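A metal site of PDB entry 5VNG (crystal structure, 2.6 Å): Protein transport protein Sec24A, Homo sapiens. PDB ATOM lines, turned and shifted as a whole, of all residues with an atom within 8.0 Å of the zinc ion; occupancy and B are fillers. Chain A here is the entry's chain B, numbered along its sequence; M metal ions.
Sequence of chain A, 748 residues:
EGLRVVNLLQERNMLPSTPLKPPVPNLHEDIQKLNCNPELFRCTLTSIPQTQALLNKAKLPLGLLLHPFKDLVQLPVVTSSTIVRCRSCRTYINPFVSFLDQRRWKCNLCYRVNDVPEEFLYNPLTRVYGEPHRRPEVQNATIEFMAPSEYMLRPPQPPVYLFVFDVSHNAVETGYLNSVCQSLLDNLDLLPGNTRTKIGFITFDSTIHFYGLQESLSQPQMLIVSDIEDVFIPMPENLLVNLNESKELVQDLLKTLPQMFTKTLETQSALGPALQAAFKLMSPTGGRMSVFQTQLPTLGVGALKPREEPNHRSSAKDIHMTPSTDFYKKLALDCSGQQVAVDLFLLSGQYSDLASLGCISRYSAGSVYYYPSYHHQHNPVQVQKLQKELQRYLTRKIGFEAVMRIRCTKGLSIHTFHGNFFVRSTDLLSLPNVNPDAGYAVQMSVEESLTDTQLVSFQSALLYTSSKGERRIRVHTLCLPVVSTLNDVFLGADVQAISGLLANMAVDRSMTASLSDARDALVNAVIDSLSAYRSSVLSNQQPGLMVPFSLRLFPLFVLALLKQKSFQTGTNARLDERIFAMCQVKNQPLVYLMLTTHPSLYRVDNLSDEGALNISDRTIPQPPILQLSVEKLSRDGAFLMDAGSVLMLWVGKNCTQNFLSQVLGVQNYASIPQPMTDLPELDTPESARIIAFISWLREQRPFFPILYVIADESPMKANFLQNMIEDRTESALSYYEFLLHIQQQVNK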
ATOM      1  N   ARG A  85      16.483 -23.710  29.783  1.00  0.00           N
ATOM      2  CA  ARG A  85      15.325 -23.227  29.052  1.00  0.00           C
ATOM      3  C   ARG A  85      14.938 -24.246  27.985  1.00  0.00           C
ATOM      4  O   ARG A  85      15.749 -25.081  27.581  1.00  0.00           O
ATOM      5  CB  ARG A  85      15.591 -21.866  28.392  1.00  0.00           C
ATOM      6  CG  ARG A  85      16.068 -20.795  29.367  1.00  0.00           C
ATOM      7  CD  ARG A  85      16.349 -19.487  28.654  1.00  0.00           C
ATOM      8  NE  ARG A  85      15.119 -18.812  28.245  1.00  0.00           N
ATOM      9  CZ  ARG A  85      15.080 -17.625  27.648  1.00  0.00           C
ATOM     10  NH1 ARG A  85      16.215 -16.982  27.381  1.00  0.00           N
ATOM     11  NH2 ARG A  85      13.918 -17.085  27.321  1.00  0.00           N
ATOM     12  N   CYS A  86      13.695 -24.156  27.528  1.00  0.00           N
ATOM     13  CA  CYS A  86      13.223 -25.044  26.470  1.00  0.00           C
ATOM     14  C   CYS A  86      13.926 -24.699  25.160  1.00  0.00           C
ATOM     15  O   CYS A  86      14.245 -23.543  24.884  1.00  0.00           O
ATOM     16  CB  CYS A  86      11.708 -24.940  26.316  1.00  0.00           C
ATOM     17  SG  CYS A  86      10.998 -25.893  24.939  1.00  0.00           S
ATOM     18  N   ARG A  87      14.148 -25.732  24.347  1.00  0.00           N
ATOM     19  CA  ARG A  87      14.894 -25.569  23.102  1.00  0.00           C
ATOM     20  C   ARG A  87      14.111 -24.842  22.016  1.00  0.00           C
ATOM     21  O   ARG A  87      14.697 -24.480  20.997  1.00  0.00           O
ATOM     22  CB  ARG A  87      15.336 -26.939  22.587  1.00  0.00           C
ATOM     23  CG  ARG A  87      16.691 -26.951  21.903  1.00  0.00           C
ATOM     24  CD  ARG A  87      16.987 -28.303  21.297  1.00  0.00           C
ATOM     25  NE  ARG A  87      18.392 -28.448  20.931  1.00  0.00           N
ATOM     26  CZ  ARG A  87      18.887 -29.491  20.275  1.00  0.00           C
ATOM     27  NH1 ARG A  87      18.084 -30.470  19.880  1.00  0.00           N
ATOM     28  NH2 ARG A  87      20.183 -29.547  19.989  1.00  0.00           N
ATOM     29  N   SER A  88      12.803 -24.627  22.204  1.00  0.00           N
ATOM     30  CA  SER A  88      11.976 -23.994  21.178  1.00  0.00           C
ATOM     31  C   SER A  88      11.498 -22.613  21.632  1.00  0.00           C
ATOM     32  O   SER A  88      12.002 -21.610  21.148  1.00  0.00           O
ATOM     33  CB  SER A  88      10.802 -24.899  20.824  1.00  0.00           C
ATOM     34  OG  SER A  88      11.245 -26.056  20.144  1.00  0.00           O
ATOM     35  N   CYS A  89      10.526 -22.554  22.539  1.00  0.00           N
ATOM     36  CA  CYS A  89       9.968 -21.277  22.985  1.00  0.00           C
ATOM     37  C   CYS A  89      10.788 -20.634  24.097  1.00  0.00           C
ATOM     38  O   CYS A  89      10.353 -19.615  24.648  1.00  0.00           O
ATOM     39  CB  CYS A  89       8.523 -21.456  23.453  1.00  0.00           C
ATOM     40  SG  CYS A  89       8.318 -22.563  24.876  1.00  0.00           S
ATOM     41  N   ARG A  90      11.947 -21.196  24.435  1.00  0.00           N
ATOM     42  CA  ARG A  90      12.857 -20.637  25.435  1.00  0.00           C
ATOM     43  C   ARG A  90      12.170 -20.482  26.795  1.00  0.00           C
ATOM     44  O   ARG A  90      12.533 -19.614  27.591  1.00  0.00           O
ATOM     45  CB  ARG A  90      13.447 -19.308  24.970  1.00  0.00           C
ATOM     46  CG  ARG A  90      14.307 -19.428  23.723  1.00  0.00           C
ATOM     47  CD  ARG A  90      15.671 -20.017  24.046  1.00  0.00           C
ATOM     48  NE  ARG A  90      16.531 -19.061  24.742  1.00  0.00           N
ATOM     49  CZ  ARG A  90      17.743 -19.355  25.209  1.00  0.00           C
ATOM     50  NH1 ARG A  90      18.232 -20.574  25.048  1.00  0.00           N
ATOM     51  NH2 ARG A  90      18.461 -18.424  25.830  1.00  0.00           N
ATOM     52  N   THR A  91      11.181 -21.325  27.080  1.00  0.00           N
ATOM     53  CA  THR A  91      10.492 -21.282  28.364  1.00  0.00           C
ATOM     54  C   THR A  91      11.421 -21.781  29.465  1.00  0.00           C
ATOM     55  O   THR A  91      12.068 -22.835  29.324  1.00  0.00           O
ATOM     56  CB  THR A  91       9.225 -22.125  28.317  1.00  0.00           C
ATOM     57  OG1 THR A  91       8.311 -21.579  27.359  1.00  0.00           O
ATOM     58  CG2 THR A  91       8.540 -22.170  29.685  1.00  0.00           C
ATOM     59  N   TYR A  92      11.506 -21.028  30.558  1.00  0.00           N
ATOM     60  CA  TYR A  92      12.341 -21.434  31.683  1.00  0.00           C
ATOM     61  C   TYR A  92      11.729 -22.660  32.366  1.00  0.00           C
ATOM     62  O   TYR A  92      10.510 -22.733  32.566  1.00  0.00           O
ATOM     63  CB  TYR A  92      12.477 -20.278  32.673  1.00  0.00           C
ATOM     64  CG  TYR A  92      13.202 -19.090  32.098  1.00  0.00           C
ATOM     65  CD1 TYR A  92      12.525 -18.124  31.355  1.00  0.00           C
ATOM     66  CD2 TYR A  92      14.564 -18.924  32.284  1.00  0.00           C
ATOM     67  CE1 TYR A  92      13.186 -17.025  30.828  1.00  0.00           C
ATOM     68  CE2 TYR A  92      15.238 -17.831  31.758  1.00  0.00           C
ATOM     69  CZ  TYR A  92      14.551 -16.888  31.030  1.00  0.00           C
ATOM     70  OH  TYR A  92      15.223 -15.817  30.514  1.00  0.00           O
ATOM     71  N   TRP A 105      12.822 -33.832  29.915  1.00  0.00           N
ATOM     72  CA  TRP A 105      11.629 -33.162  30.416  1.00  0.00           C
ATOM     73  C   TRP A 105      10.802 -32.610  29.264  1.00  0.00           C
ATOM     74  O   TRP A 105      11.344 -32.127  28.264  1.00  0.00           O
ATOM     75  CB  TRP A 105      11.993 -32.029  31.394  1.00  0.00           C
ATOM     76  CG  TRP A 105      12.813 -30.913  30.803  1.00  0.00           C
ATOM     77  CD1 TRP A 105      14.154 -30.921  30.571  1.00  0.00           C
ATOM     78  CD2 TRP A 105      12.341 -29.616  30.417  1.00  0.00           C
ATOM     79  NE1 TRP A 105      14.547 -29.711  30.050  1.00  0.00           N
ATOM     80  CE2 TRP A 105      13.455 -28.898  29.947  1.00  0.00           C
ATOM     81  CE3 TRP A 105      11.085 -28.994  30.421  1.00  0.00           C
ATOM     82  CZ2 TRP A 105      13.348 -27.589  29.472  1.00  0.00           C
ATOM     83  CZ3 TRP A 105      10.993 -27.705  29.946  1.00  0.00           C
ATOM     84  CH2 TRP A 105      12.113 -27.007  29.482  1.00  0.00           C
ATOM     85  N   LYS A 106       9.481 -32.682  29.407  1.00  0.00           N
ATOM     86  CA  LYS A 106       8.544 -32.201  28.409  1.00  0.00           C
ATOM     87  C   LYS A 106       8.110 -30.789  28.765  1.00  0.00           C
ATOM     88  O   LYS A 106       7.612 -30.541  29.870  1.00  0.00           O
ATOM     89  CB  LYS A 106       7.327 -33.121  28.305  1.00  0.00           C
ATOM     90  CG  LYS A 106       6.189 -32.554  27.470  1.00  0.00           C
ATOM     91  CD  LYS A 106       5.121 -33.596  27.185  1.00  0.00           C
ATOM     92  CE  LYS A 106       5.648 -34.675  26.245  1.00  0.00           C
ATOM     93  NZ  LYS A 106       4.622 -35.696  25.936  1.00  0.00           N
ATOM     94  N   CYS A 107       8.304 -29.850  27.832  1.00  0.00           N
ATOM     95  CA  CYS A 107       7.947 -28.458  28.073  1.00  0.00           C
ATOM     96  C   CYS A 107       6.445 -28.328  28.259  1.00  0.00           C
ATOM     97  O   CYS A 107       5.662 -28.870  27.470  1.00  0.00           O
ATOM     98  CB  CYS A 107       8.441 -27.583  26.912  1.00  0.00           C
ATOM     99  SG  CYS A 107       8.105 -25.792  27.036  1.00  0.00           S
ATOM    100  N   ASN A 108       6.039 -27.622  29.309  1.00  0.00           N
ATOM    101  CA  ASN A 108       4.616 -27.478  29.621  1.00  0.00           C
ATOM    102  C   ASN A 108       3.944 -26.387  28.797  1.00  0.00           C
ATOM    103  O   ASN A 108       2.739 -26.165  28.984  1.00  0.00           O
ATOM    104  CB  ASN A 108       4.442 -27.183  31.111  1.00  0.00           C
ATOM    105  CG  ASN A 108       5.254 -25.997  31.580  1.00  0.00           C
ATOM    106  OD1 ASN A 108       6.307 -25.693  31.026  1.00  0.00           O
ATOM    107  ND2 ASN A 108       4.776 -25.322  32.616  1.00  0.00           N
ATOM    108  N   LEU A 109       4.659 -25.725  27.887  1.00  0.00           N
ATOM    109  CA  LEU A 109       4.068 -24.701  27.045  1.00  0.00           C
ATOM    110  C   LEU A 109       4.077 -25.041  25.559  1.00  0.00           C
ATOM    111  O   LEU A 109       3.179 -24.594  24.847  1.00  0.00           O
ATOM    112  CB  LEU A 109       4.778 -23.349  27.256  1.00  0.00           C
ATOM    113  CG  LEU A 109       4.289 -22.502  28.427  1.00  0.00           C
ATOM    114  CD1 LEU A 109       4.716 -23.074  29.768  1.00  0.00           C
ATOM    115  CD2 LEU A 109       4.776 -21.077  28.281  1.00  0.00           C
ATOM    116  N   CYS A 110       5.054 -25.807  25.077  1.00  0.00           N
ATOM    117  CA  CYS A 110       5.087 -26.240  23.687  1.00  0.00           C
ATOM    118  C   CYS A 110       5.177 -27.759  23.534  1.00  0.00           C
ATOM    119  O   CYS A 110       5.282 -28.240  22.405  1.00  0.00           O
ATOM    120  CB  CYS A 110       6.252 -25.584  22.941  1.00  0.00           C
ATOM    121  SG  CYS A 110       7.881 -26.260  23.339  1.00  0.00           S
ATOM    122  N   TYR A 111       5.153 -28.508  24.639  1.00  0.00           N
ATOM    123  CA  TYR A 111       5.070 -29.970  24.628  1.00  0.00           C
ATOM    124  C   TYR A 111       6.307 -30.631  24.021  1.00  0.00           C
ATOM    125  O   TYR A 111       6.276 -31.810  23.686  1.00  0.00           O
ATOM    126  CB  TYR A 111       3.812 -30.445  23.897  1.00  0.00           C
ATOM    127  CG  TYR A 111       2.543 -29.747  24.333  1.00  0.00           C
ATOM    128  CD1 TYR A 111       2.258 -29.549  25.679  1.00  0.00           C
ATOM    129  CD2 TYR A 111       1.644 -29.256  23.386  1.00  0.00           C
ATOM    130  CE1 TYR A 111       1.087 -28.900  26.071  1.00  0.00           C
ATOM    131  CE2 TYR A 111       0.487 -28.613  23.779  1.00  0.00           C
ATOM    132  CZ  TYR A 111       0.214 -28.441  25.119  1.00  0.00           C
ATOM    133  OH  TYR A 111      -0.946 -27.789  25.489  1.00  0.00           O
ATOM    134  N   ARG A 112       7.410 -29.890  23.889  1.00  0.00           N
ATOM    135  CA  ARG A 112       8.627 -30.441  23.320  1.00  0.00           C
ATOM    136  C   ARG A 112       9.489 -31.071  24.408  1.00  0.00           C
ATOM    137  O   ARG A 112       9.563 -30.563  25.534  1.00  0.00           O
ATOM    138  CB  ARG A 112       9.423 -29.358  22.574  1.00  0.00           C
ATOM    139  CG  ARG A 112      10.812 -29.782  22.140  1.00  0.00           C
ATOM    140  CD  ARG A 112      11.212 -29.129  20.831  1.00  0.00           C
ATOM    141  NE  ARG A 112      12.627 -29.346  20.527  1.00  0.00           N
ATOM    142  CZ  ARG A 112      13.204 -28.975  19.391  1.00  0.00           C
ATOM    143  NH1 ARG A 112      12.497 -28.371  18.446  1.00  0.00           N
ATOM    144  NH2 ARG A 112      14.498 -29.206  19.196  1.00  0.00           N
ATOM    145  N   VAL A 113      10.128 -32.183  24.071  1.00  0.00           N
ATOM    146  CA  VAL A 113      11.011 -32.890  24.989  1.00  0.00           C
ATOM    147  C   VAL A 113      12.407 -32.281  24.909  1.00  0.00           C
ATOM    148  O   VAL A 113      12.923 -32.034  23.813  1.00  0.00           O
ATOM    149  CB  VAL A 113      11.045 -34.395  24.656  1.00  0.00           C
ATOM    150  CG1 VAL A 113      11.711 -35.176  25.785  1.00  0.00           C
ATOM    151  CG2 VAL A 113       9.648 -34.906  24.391  1.00  0.00           C
ATOM    152  N   ASN A 114      13.017 -32.049  26.066  1.00  0.00           N
ATOM    153  CA  ASN A 114      14.320 -31.394  26.142  1.00  0.00           C
ATOM    154  C   ASN A 114      15.292 -32.242  26.951  1.00  0.00           C
ATOM    155  O   ASN A 114      14.897 -32.987  27.849  1.00  0.00           O
ATOM    156  CB  ASN A 114      14.209 -30.011  26.797  1.00  0.00           C
ATOM    157  CG  ASN A 114      13.497 -29.010  25.918  1.00  0.00           C
ATOM    158  OD1 ASN A 114      14.144 -28.228  25.211  1.00  0.00           O
ATOM    159  ND2 ASN A 114      12.172 -29.020  25.947  1.00  0.00           N
ATOM    160  N   ARG A 407       4.780 -15.635  28.598  1.00  0.00           N
ATOM    161  CA  ARG A 407       4.519 -16.816  27.792  1.00  0.00           C
ATOM    162  C   ARG A 407       3.354 -17.601  28.357  1.00  0.00           C
ATOM    163  O   ARG A 407       3.143 -17.659  29.576  1.00  0.00           O
ATOM    164  CB  ARG A 407       5.759 -17.716  27.720  1.00  0.00           C
ATOM    165  CG  ARG A 407       6.942 -17.129  26.983  1.00  0.00           C
ATOM    166  CD  ARG A 407       8.101 -18.122  26.968  1.00  0.00           C
ATOM    167  NE  ARG A 407       9.263 -17.617  26.255  1.00  0.00           N
ATOM    168  CZ  ARG A 407      10.216 -16.858  26.811  1.00  0.00           C
ATOM    169  NH1 ARG A 407      10.122 -16.522  28.085  1.00  0.00           N
ATOM    170  NH2 ARG A 407      11.243 -16.443  26.079  1.00  0.00           N
HETATM  171 ZN    ZN M   1       8.927 -24.870  24.843  1.00  0.00          ZN
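Within 4 Å of the zinc ion: Cys 86, Cys 89, Cys 107 and Cys 110. The nearest printed residue that does not touch the zinc ion is Thr 91 (4.2 Å).
The side-chain sulfur (SG) of Cys 110 lies close to the backbone NH (N) of Arg 112 (3.7 Å). The backbone NH (N) of Cys 86 is in hydrogen-bond range of the backbone carbonyl oxygen (O) of Thr 91 (2.8 Å). SG of Cys 86 sits close to N of Ser 88 (3.5 Å). The side-chain sulfur (SG) of Cys 86 lies close to the side-chain amide nitrogen (ND2) of Asn 114 (3.5 Å). SG of Cys 89 sits close to OG1 of Thr 91 (2.7 Å). The backbone carbonyl oxygen (O) of Cys 89 lies within hydrogen-bond range of the guanidinium group (NE) of Arg 407 (2.8 Å). N of Leu 109 lies close to SG of Cys 107. N of Cys 107 sits at hydrogen-bond distance from O of Arg 112, at 2.7 Å.
The zinc ion is bound by SG of Cys 110 (2.3 Å), SG of Cys 86 (2.3 Å), SG of Cys 89 (2.4 Å) and SG of Cys 107 (2.5 Å). The zinc ion has four donor atoms within binding distance.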
